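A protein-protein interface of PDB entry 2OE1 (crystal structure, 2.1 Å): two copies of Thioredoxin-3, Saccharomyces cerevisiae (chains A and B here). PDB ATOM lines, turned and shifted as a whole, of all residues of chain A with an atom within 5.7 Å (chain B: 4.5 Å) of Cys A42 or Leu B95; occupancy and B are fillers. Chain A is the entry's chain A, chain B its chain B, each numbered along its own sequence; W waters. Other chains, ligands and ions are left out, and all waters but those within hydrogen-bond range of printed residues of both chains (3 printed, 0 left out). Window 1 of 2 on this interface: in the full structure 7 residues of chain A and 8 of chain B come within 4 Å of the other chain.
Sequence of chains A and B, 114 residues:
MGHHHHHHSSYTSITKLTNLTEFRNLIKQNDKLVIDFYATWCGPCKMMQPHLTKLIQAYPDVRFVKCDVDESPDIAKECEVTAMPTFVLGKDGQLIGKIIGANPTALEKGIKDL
The backbone NH (N) of Gly A43 lies within hydrogen-bond range of the backbone carbonyl oxygen (O) of Leu B95, at 2.9 Å.
The side-chain sulfur of Cys A42 lies within hydrogen-bond range of the side-chain sulfur of Cys A45, at 3.7 Å. The backbone carbonyl oxygen of Leu B89 sits at hydrogen-bond distance from the backbone NH of Ile B96, at 2.7 Å. O of Gly B97 lies within hydrogen-bond range of N of Leu B89.
Among the printed residues, pairs that only touch across the chains: Trp A41 with Cys B79, Trp A41 with Leu B95, Trp A41 with Gly B97, Cys A42 with Leu B95, Cys A42 with Ile B96, Gly A43 with Gln B94, Pro A44 with Gln B94 and Pro A44 with Leu B95.
Of chain B, only Leu B95 and Ile B96 come within 4 Å of Cys A42. Of chain A, only Trp A41, Cys A42, Gly A43 and Pro A44 come within 4 Å of Leu B95. Printed residues of chain A within 4 Å of Gln B94: Gly A43 and Pro A44. Printed residues of chain A within 4 Å of Ile B96: Cys A42. Phe B23 touches none of the printed residues of chain A.
Hydrophobic or aromatic side chains of chain A within 4 Å of the printed part of chain B: Trp A41 and Pro A44. Hydrophobic or aromatic side chains of chain B that line the printed part of chain A: Leu B95. Among the printed residues, 9 pairs touch across the chains.
No position is printed for both chains.
Water W3 lies within hydrogen-bond range of the backbone NH (N) of Leu B95, the backbone carbonyl oxygen (O) of Trp A41 and the backbone NH (N) of Gly A43. Water W1 lies within hydrogen-bond range of O of Ile B96 (2.6 Å), O of Met A84 (2.7 Å) and SG of Cys A42 (3.6 Å). Water W2 lies within hydrogen-bond range of the backbone carbonyl oxygen of Ile B96 (2.7 Å) and the backbone NH of Met A84 (2.8 Å).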
ATOM      1  N   ALA A  39     -31.877  28.192  10.675  1.00  0.00           N
ATOM      2  CA  ALA A  39     -31.872  26.880  10.027  1.00  0.00           C
ATOM      3  C   ALA A  39     -30.414  26.451   9.962  1.00  0.00           C
ATOM      4  O   ALA A  39     -29.525  27.288   9.725  1.00  0.00           O
ATOM      5  CB  ALA A  39     -32.507  26.957   8.631  1.00  0.00           C
ATOM      6  N   THR A  40     -30.149  25.184  10.254  1.00  0.00           N
ATOM      7  CA  THR A  40     -28.775  24.656  10.267  1.00  0.00           C
ATOM      8  C   THR A  40     -28.059  24.723   8.909  1.00  0.00           C
ATOM      9  O   THR A  40     -26.851  24.884   8.871  1.00  0.00           O
ATOM     10  CB  THR A  40     -28.721  23.192  10.797  1.00  0.00           C
ATOM     11  OG1 THR A  40     -29.617  22.383  10.032  1.00  0.00           O
ATOM     12  CG2 THR A  40     -29.112  23.104  12.300  1.00  0.00           C
ATOM     13  N   TRP A  41     -28.781  24.602   7.793  1.00  0.00           N
ATOM     14  CA  TRP A  41     -28.135  24.636   6.459  1.00  0.00           C
ATOM     15  C   TRP A  41     -27.853  26.088   5.997  1.00  0.00           C
ATOM     16  O   TRP A  41     -27.184  26.306   4.986  1.00  0.00           O
ATOM     17  CB  TRP A  41     -29.007  23.896   5.429  1.00  0.00           C
ATOM     18  CG  TRP A  41     -30.464  24.330   5.572  1.00  0.00           C
ATOM     19  CD1 TRP A  41     -31.440  23.713   6.321  1.00  0.00           C
ATOM     20  CD2 TRP A  41     -31.068  25.524   5.030  1.00  0.00           C
ATOM     21  NE1 TRP A  41     -32.606  24.449   6.272  1.00  0.00           N
ATOM     22  CE2 TRP A  41     -32.403  25.561   5.489  1.00  0.00           C
ATOM     23  CE3 TRP A  41     -30.599  26.579   4.221  1.00  0.00           C
ATOM     24  CZ2 TRP A  41     -33.280  26.584   5.137  1.00  0.00           C
ATOM     25  CZ3 TRP A  41     -31.474  27.595   3.890  1.00  0.00           C
ATOM     26  CH2 TRP A  41     -32.803  27.587   4.343  1.00  0.00           C
ATOM     27  N   CYS A  42     -28.348  27.083   6.745  1.00  0.00           N
ATOM     28  CA  CYS A  42     -28.416  28.474   6.258  1.00  0.00           C
ATOM     29  C   CYS A  42     -27.165  29.297   6.604  1.00  0.00           C
ATOM     30  O   CYS A  42     -26.844  29.466   7.785  1.00  0.00           O
ATOM     31  CB  CYS A  42     -29.678  29.137   6.814  1.00  0.00           C
ATOM     32  SG  CYS A  42     -29.981  30.844   6.279  1.00  0.00           S
ATOM     33  N   GLY A  43     -26.475  29.812   5.581  1.00  0.00           N
ATOM     34  CA  GLY A  43     -25.172  30.476   5.764  1.00  0.00           C
ATOM     35  C   GLY A  43     -25.177  31.772   6.583  1.00  0.00           C
ATOM     36  O   GLY A  43     -24.265  31.999   7.393  1.00  0.00           O
ATOM     37  N   PRO A  44     -26.153  32.664   6.339  1.00  0.00           N
ATOM     38  CA  PRO A  44     -26.312  33.822   7.231  1.00  0.00           C
ATOM     39  C   PRO A  44     -26.591  33.481   8.694  1.00  0.00           C
ATOM     40  O   PRO A  44     -26.176  34.235   9.581  1.00  0.00           O
ATOM     41  CB  PRO A  44     -27.458  34.620   6.567  1.00  0.00           C
ATOM     42  CG  PRO A  44     -27.310  34.274   5.095  1.00  0.00           C
ATOM     43  CD  PRO A  44     -27.038  32.768   5.167  1.00  0.00           C
ATOM     44  N   CYS A  45     -27.256  32.354   8.959  1.00  0.00           N
ATOM     45  CA  CYS A  45     -27.453  31.900  10.341  1.00  0.00           C
ATOM     46  C   CYS A  45     -26.117  31.511  10.973  1.00  0.00           C
ATOM     47  O   CYS A  45     -25.774  31.960  12.099  1.00  0.00           O
ATOM     48  CB  CYS A  45     -28.460  30.731  10.391  1.00  0.00           C
ATOM     49  SG  CYS A  45     -30.138  31.203   9.931  1.00  0.00           S
ATOM     50  N   LYS A  46     -25.343  30.713  10.228  1.00  0.00           N
ATOM     51  CA  LYS A  46     -24.030  30.267  10.673  1.00  0.00           C
ATOM     52  C   LYS A  46     -23.101  31.452  10.925  1.00  0.00           C
ATOM     53  O   LYS A  46     -22.381  31.459  11.941  1.00  0.00           O
ATOM     54  CB  LYS A  46     -23.382  29.322   9.662  1.00  0.00           C
ATOM     55  CG  LYS A  46     -24.160  28.077   9.379  1.00  0.00           C
ATOM     56  CD  LYS A  46     -23.347  27.157   8.449  1.00  0.00           C
ATOM     57  CE  LYS A  46     -24.198  26.006   7.951  1.00  0.00           C
ATOM     58  NZ  LYS A  46     -23.371  24.913   7.385  1.00  0.00           N
ATOM     59  N   MET A  47     -23.130  32.434  10.011  1.00  0.00           N
ATOM     60  CA  MET A  47     -22.354  33.684  10.150  1.00  0.00           C
ATOM     61  C   MET A  47     -22.691  34.418  11.447  1.00  0.00           C
ATOM     62  O   MET A  47     -21.808  34.967  12.098  1.00  0.00           O
ATOM     63  CB  MET A  47     -22.563  34.623   8.940  1.00  0.00           C
ATOM     64  CG  MET A  47     -21.834  35.988   9.013  1.00  0.00           C
ATOM     65  SD  MET A  47     -22.647  37.325  10.001  1.00  0.00           S
ATOM     66  CE  MET A  47     -23.089  38.520   8.724  1.00  0.00           C
ATOM     67  N   MET A  84     -34.285  33.723   7.316  1.00  0.00           N
ATOM     68  CA  MET A  84     -33.313  33.252   8.314  1.00  0.00           C
ATOM     69  C   MET A  84     -32.015  34.054   8.225  1.00  0.00           C
ATOM     70  O   MET A  84     -31.521  34.288   7.141  1.00  0.00           O
ATOM     71  CB  MET A  84     -32.861  31.813   8.075  1.00  0.00           C
ATOM     72  CG  MET A  84     -33.843  30.831   7.591  1.00  0.00           C
ATOM     73  SD  MET A  84     -34.933  30.696   8.954  1.00  0.00           S
ATOM     74  CE  MET A  84     -36.330  30.742   7.866  1.00  0.00           C
ATOM     75  N   PRO A  85     -31.437  34.440   9.375  1.00  0.00           N
ATOM     76  CA  PRO A  85     -32.021  34.352  10.706  1.00  0.00           C
ATOM     77  C   PRO A  85     -33.039  35.464  10.941  1.00  0.00           C
ATOM     78  O   PRO A  85     -32.944  36.525  10.322  1.00  0.00           O
ATOM     79  CB  PRO A  85     -30.812  34.550  11.616  1.00  0.00           C
ATOM     80  CG  PRO A  85     -29.934  35.454  10.842  1.00  0.00           C
ATOM     81  CD  PRO A  85     -30.090  35.038   9.404  1.00  0.00           C
ATOM     82  N   PHE B  23     -22.356  18.718  -3.810  1.00  0.00           N
ATOM     83  CA  PHE B  23     -23.374  19.691  -3.389  1.00  0.00           C
ATOM     84  C   PHE B  23     -22.698  20.933  -2.754  1.00  0.00           C
ATOM     85  O   PHE B  23     -22.916  22.064  -3.176  1.00  0.00           O
ATOM     86  CB  PHE B  23     -24.351  18.933  -2.437  1.00  0.00           C
ATOM     87  CG  PHE B  23     -25.149  19.808  -1.482  1.00  0.00           C
ATOM     88  CD1 PHE B  23     -26.267  20.511  -1.916  1.00  0.00           C
ATOM     89  CD2 PHE B  23     -24.826  19.855  -0.137  1.00  0.00           C
ATOM     90  CE1 PHE B  23     -27.052  21.294  -1.009  1.00  0.00           C
ATOM     91  CE2 PHE B  23     -25.591  20.619   0.766  1.00  0.00           C
ATOM     92  CZ  PHE B  23     -26.714  21.344   0.313  1.00  0.00           C
ATOM     93  N   ILE B  27     -22.437  24.833  -4.266  1.00  0.00           N
ATOM     94  CA  ILE B  27     -22.930  25.978  -3.491  1.00  0.00           C
ATOM     95  C   ILE B  27     -21.877  27.098  -3.543  1.00  0.00           C
ATOM     96  O   ILE B  27     -22.222  28.248  -3.779  1.00  0.00           O
ATOM     97  CB  ILE B  27     -23.270  25.597  -2.023  1.00  0.00           C
ATOM     98  CG1 ILE B  27     -24.502  24.712  -1.953  1.00  0.00           C
ATOM     99  CG2 ILE B  27     -23.573  26.824  -1.190  1.00  0.00           C
ATOM    100  CD1 ILE B  27     -24.534  23.850  -0.693  1.00  0.00           C
ATOM    101  N   ILE B  35     -31.836  24.542  -5.904  1.00  0.00           N
ATOM    102  CA  ILE B  35     -31.895  23.077  -5.841  1.00  0.00           C
ATOM    103  C   ILE B  35     -33.335  22.616  -5.637  1.00  0.00           C
ATOM    104  O   ILE B  35     -34.010  22.991  -4.657  1.00  0.00           O
ATOM    105  CB  ILE B  35     -31.017  22.497  -4.700  1.00  0.00           C
ATOM    106  CG1 ILE B  35     -29.657  23.212  -4.664  1.00  0.00           C
ATOM    107  CG2 ILE B  35     -30.924  20.927  -4.789  1.00  0.00           C
ATOM    108  CD1 ILE B  35     -28.976  23.038  -3.376  1.00  0.00           C
ATOM    109  N   CYS B  79     -30.122  19.622   4.233  1.00  0.00           N
ATOM    110  CA  CYS B  79     -31.037  20.765   4.025  1.00  0.00           C
ATOM    111  C   CYS B  79     -32.374  20.684   4.785  1.00  0.00           C
ATOM    112  O   CYS B  79     -33.320  21.439   4.488  1.00  0.00           O
ATOM    113  CB  CYS B  79     -31.272  20.993   2.525  1.00  0.00           C
ATOM    114  SG  CYS B  79     -29.772  21.571   1.753  1.00  0.00           S
ATOM    115  N   VAL B  88     -34.344  25.038  -2.563  1.00  0.00           N
ATOM    116  CA  VAL B  88     -33.353  25.642  -1.681  1.00  0.00           C
ATOM    117  C   VAL B  88     -32.586  26.657  -2.543  1.00  0.00           C
ATOM    118  O   VAL B  88     -32.191  26.342  -3.663  1.00  0.00           O
ATOM    119  CB  VAL B  88     -32.453  24.533  -1.003  1.00  0.00           C
ATOM    120  CG1 VAL B  88     -31.271  25.108  -0.311  1.00  0.00           C
ATOM    121  CG2 VAL B  88     -33.274  23.664   0.002  1.00  0.00           C
ATOM    122  N   LEU B  89     -32.415  27.875  -2.030  1.00  0.00           N
ATOM    123  CA  LEU B  89     -31.794  28.950  -2.790  1.00  0.00           C
ATOM    124  C   LEU B  89     -30.448  29.342  -2.170  1.00  0.00           C
ATOM    125  O   LEU B  89     -30.305  29.427  -0.930  1.00  0.00           O
ATOM    126  CB  LEU B  89     -32.731  30.170  -2.909  1.00  0.00           C
ATOM    127  CG  LEU B  89     -34.210  30.050  -3.369  1.00  0.00           C
ATOM    128  CD1 LEU B  89     -34.764  31.390  -3.869  1.00  0.00           C
ATOM    129  CD2 LEU B  89     -34.521  28.988  -4.408  1.00  0.00           C
ATOM    130  N   GLY B  90     -29.467  29.518  -3.054  1.00  0.00           N
ATOM    131  CA  GLY B  90     -28.145  29.925  -2.688  1.00  0.00           C
ATOM    132  C   GLY B  90     -27.768  31.209  -3.421  1.00  0.00           C
ATOM    133  O   GLY B  90     -28.166  31.442  -4.573  1.00  0.00           O
ATOM    134  N   GLN B  94     -23.354  30.649  -0.511  1.00  0.00           N
ATOM    135  CA  GLN B  94     -23.979  30.049   0.678  1.00  0.00           C
ATOM    136  C   GLN B  94     -25.470  29.871   0.461  1.00  0.00           C
ATOM    137  O   GLN B  94     -26.083  30.575  -0.357  1.00  0.00           O
ATOM    138  CB  GLN B  94     -23.724  30.914   1.910  1.00  0.00           C
ATOM    139  CG  GLN B  94     -24.231  32.326   1.728  1.00  0.00           C
ATOM    140  CD  GLN B  94     -23.941  33.224   2.904  1.00  0.00           C
ATOM    141  OE1 GLN B  94     -23.411  32.790   3.928  1.00  0.00           O
ATOM    142  NE2 GLN B  94     -24.305  34.505   2.758  1.00  0.00           N
ATOM    143  N   LEU B  95     -26.062  28.943   1.199  1.00  0.00           N
ATOM    144  CA  LEU B  95     -27.500  28.754   1.101  1.00  0.00           C
ATOM    145  C   LEU B  95     -28.202  29.844   1.910  1.00  0.00           C
ATOM    146  O   LEU B  95     -27.821  30.102   3.055  1.00  0.00           O
ATOM    147  CB  LEU B  95     -27.887  27.349   1.564  1.00  0.00           C
ATOM    148  CG  LEU B  95     -27.269  26.180   0.795  1.00  0.00           C
ATOM    149  CD1 LEU B  95     -27.672  24.860   1.435  1.00  0.00           C
ATOM    150  CD2 LEU B  95     -27.675  26.283  -0.716  1.00  0.00           C
ATOM    151  N   ILE B  96     -29.225  30.483   1.320  1.00  0.00           N
ATOM    152  CA  ILE B  96     -29.917  31.609   1.988  1.00  0.00           C
ATOM    153  C   ILE B  96     -31.404  31.433   2.316  1.00  0.00           C
ATOM    154  O   ILE B  96     -31.927  32.111   3.229  1.00  0.00           O
ATOM    155  CB  ILE B  96     -29.762  32.927   1.181  1.00  0.00           C
ATOM    156  CG1 ILE B  96     -30.333  32.727  -0.236  1.00  0.00           C
ATOM    157  CG2 ILE B  96     -28.247  33.426   1.199  1.00  0.00           C
ATOM    158  CD1 ILE B  96     -31.077  33.914  -0.749  1.00  0.00           C
ATOM    159  N   GLY B  97     -32.094  30.553   1.588  1.00  0.00           N
ATOM    160  CA  GLY B  97     -33.540  30.394   1.742  1.00  0.00           C
ATOM    161  C   GLY B  97     -34.088  29.082   1.207  1.00  0.00           C
ATOM    162  O   GLY B  97     -33.409  28.337   0.511  1.00  0.00           O
HETATM  163  O   HOH W   1     -30.625  33.947   4.615  1.00  0.00           O
HETATM  164  O   HOH W   2     -34.107  32.947   4.587  1.00  0.00           O
HETATM  165  O   HOH W   3     -24.895  27.833   3.222  1.00  0.00           O
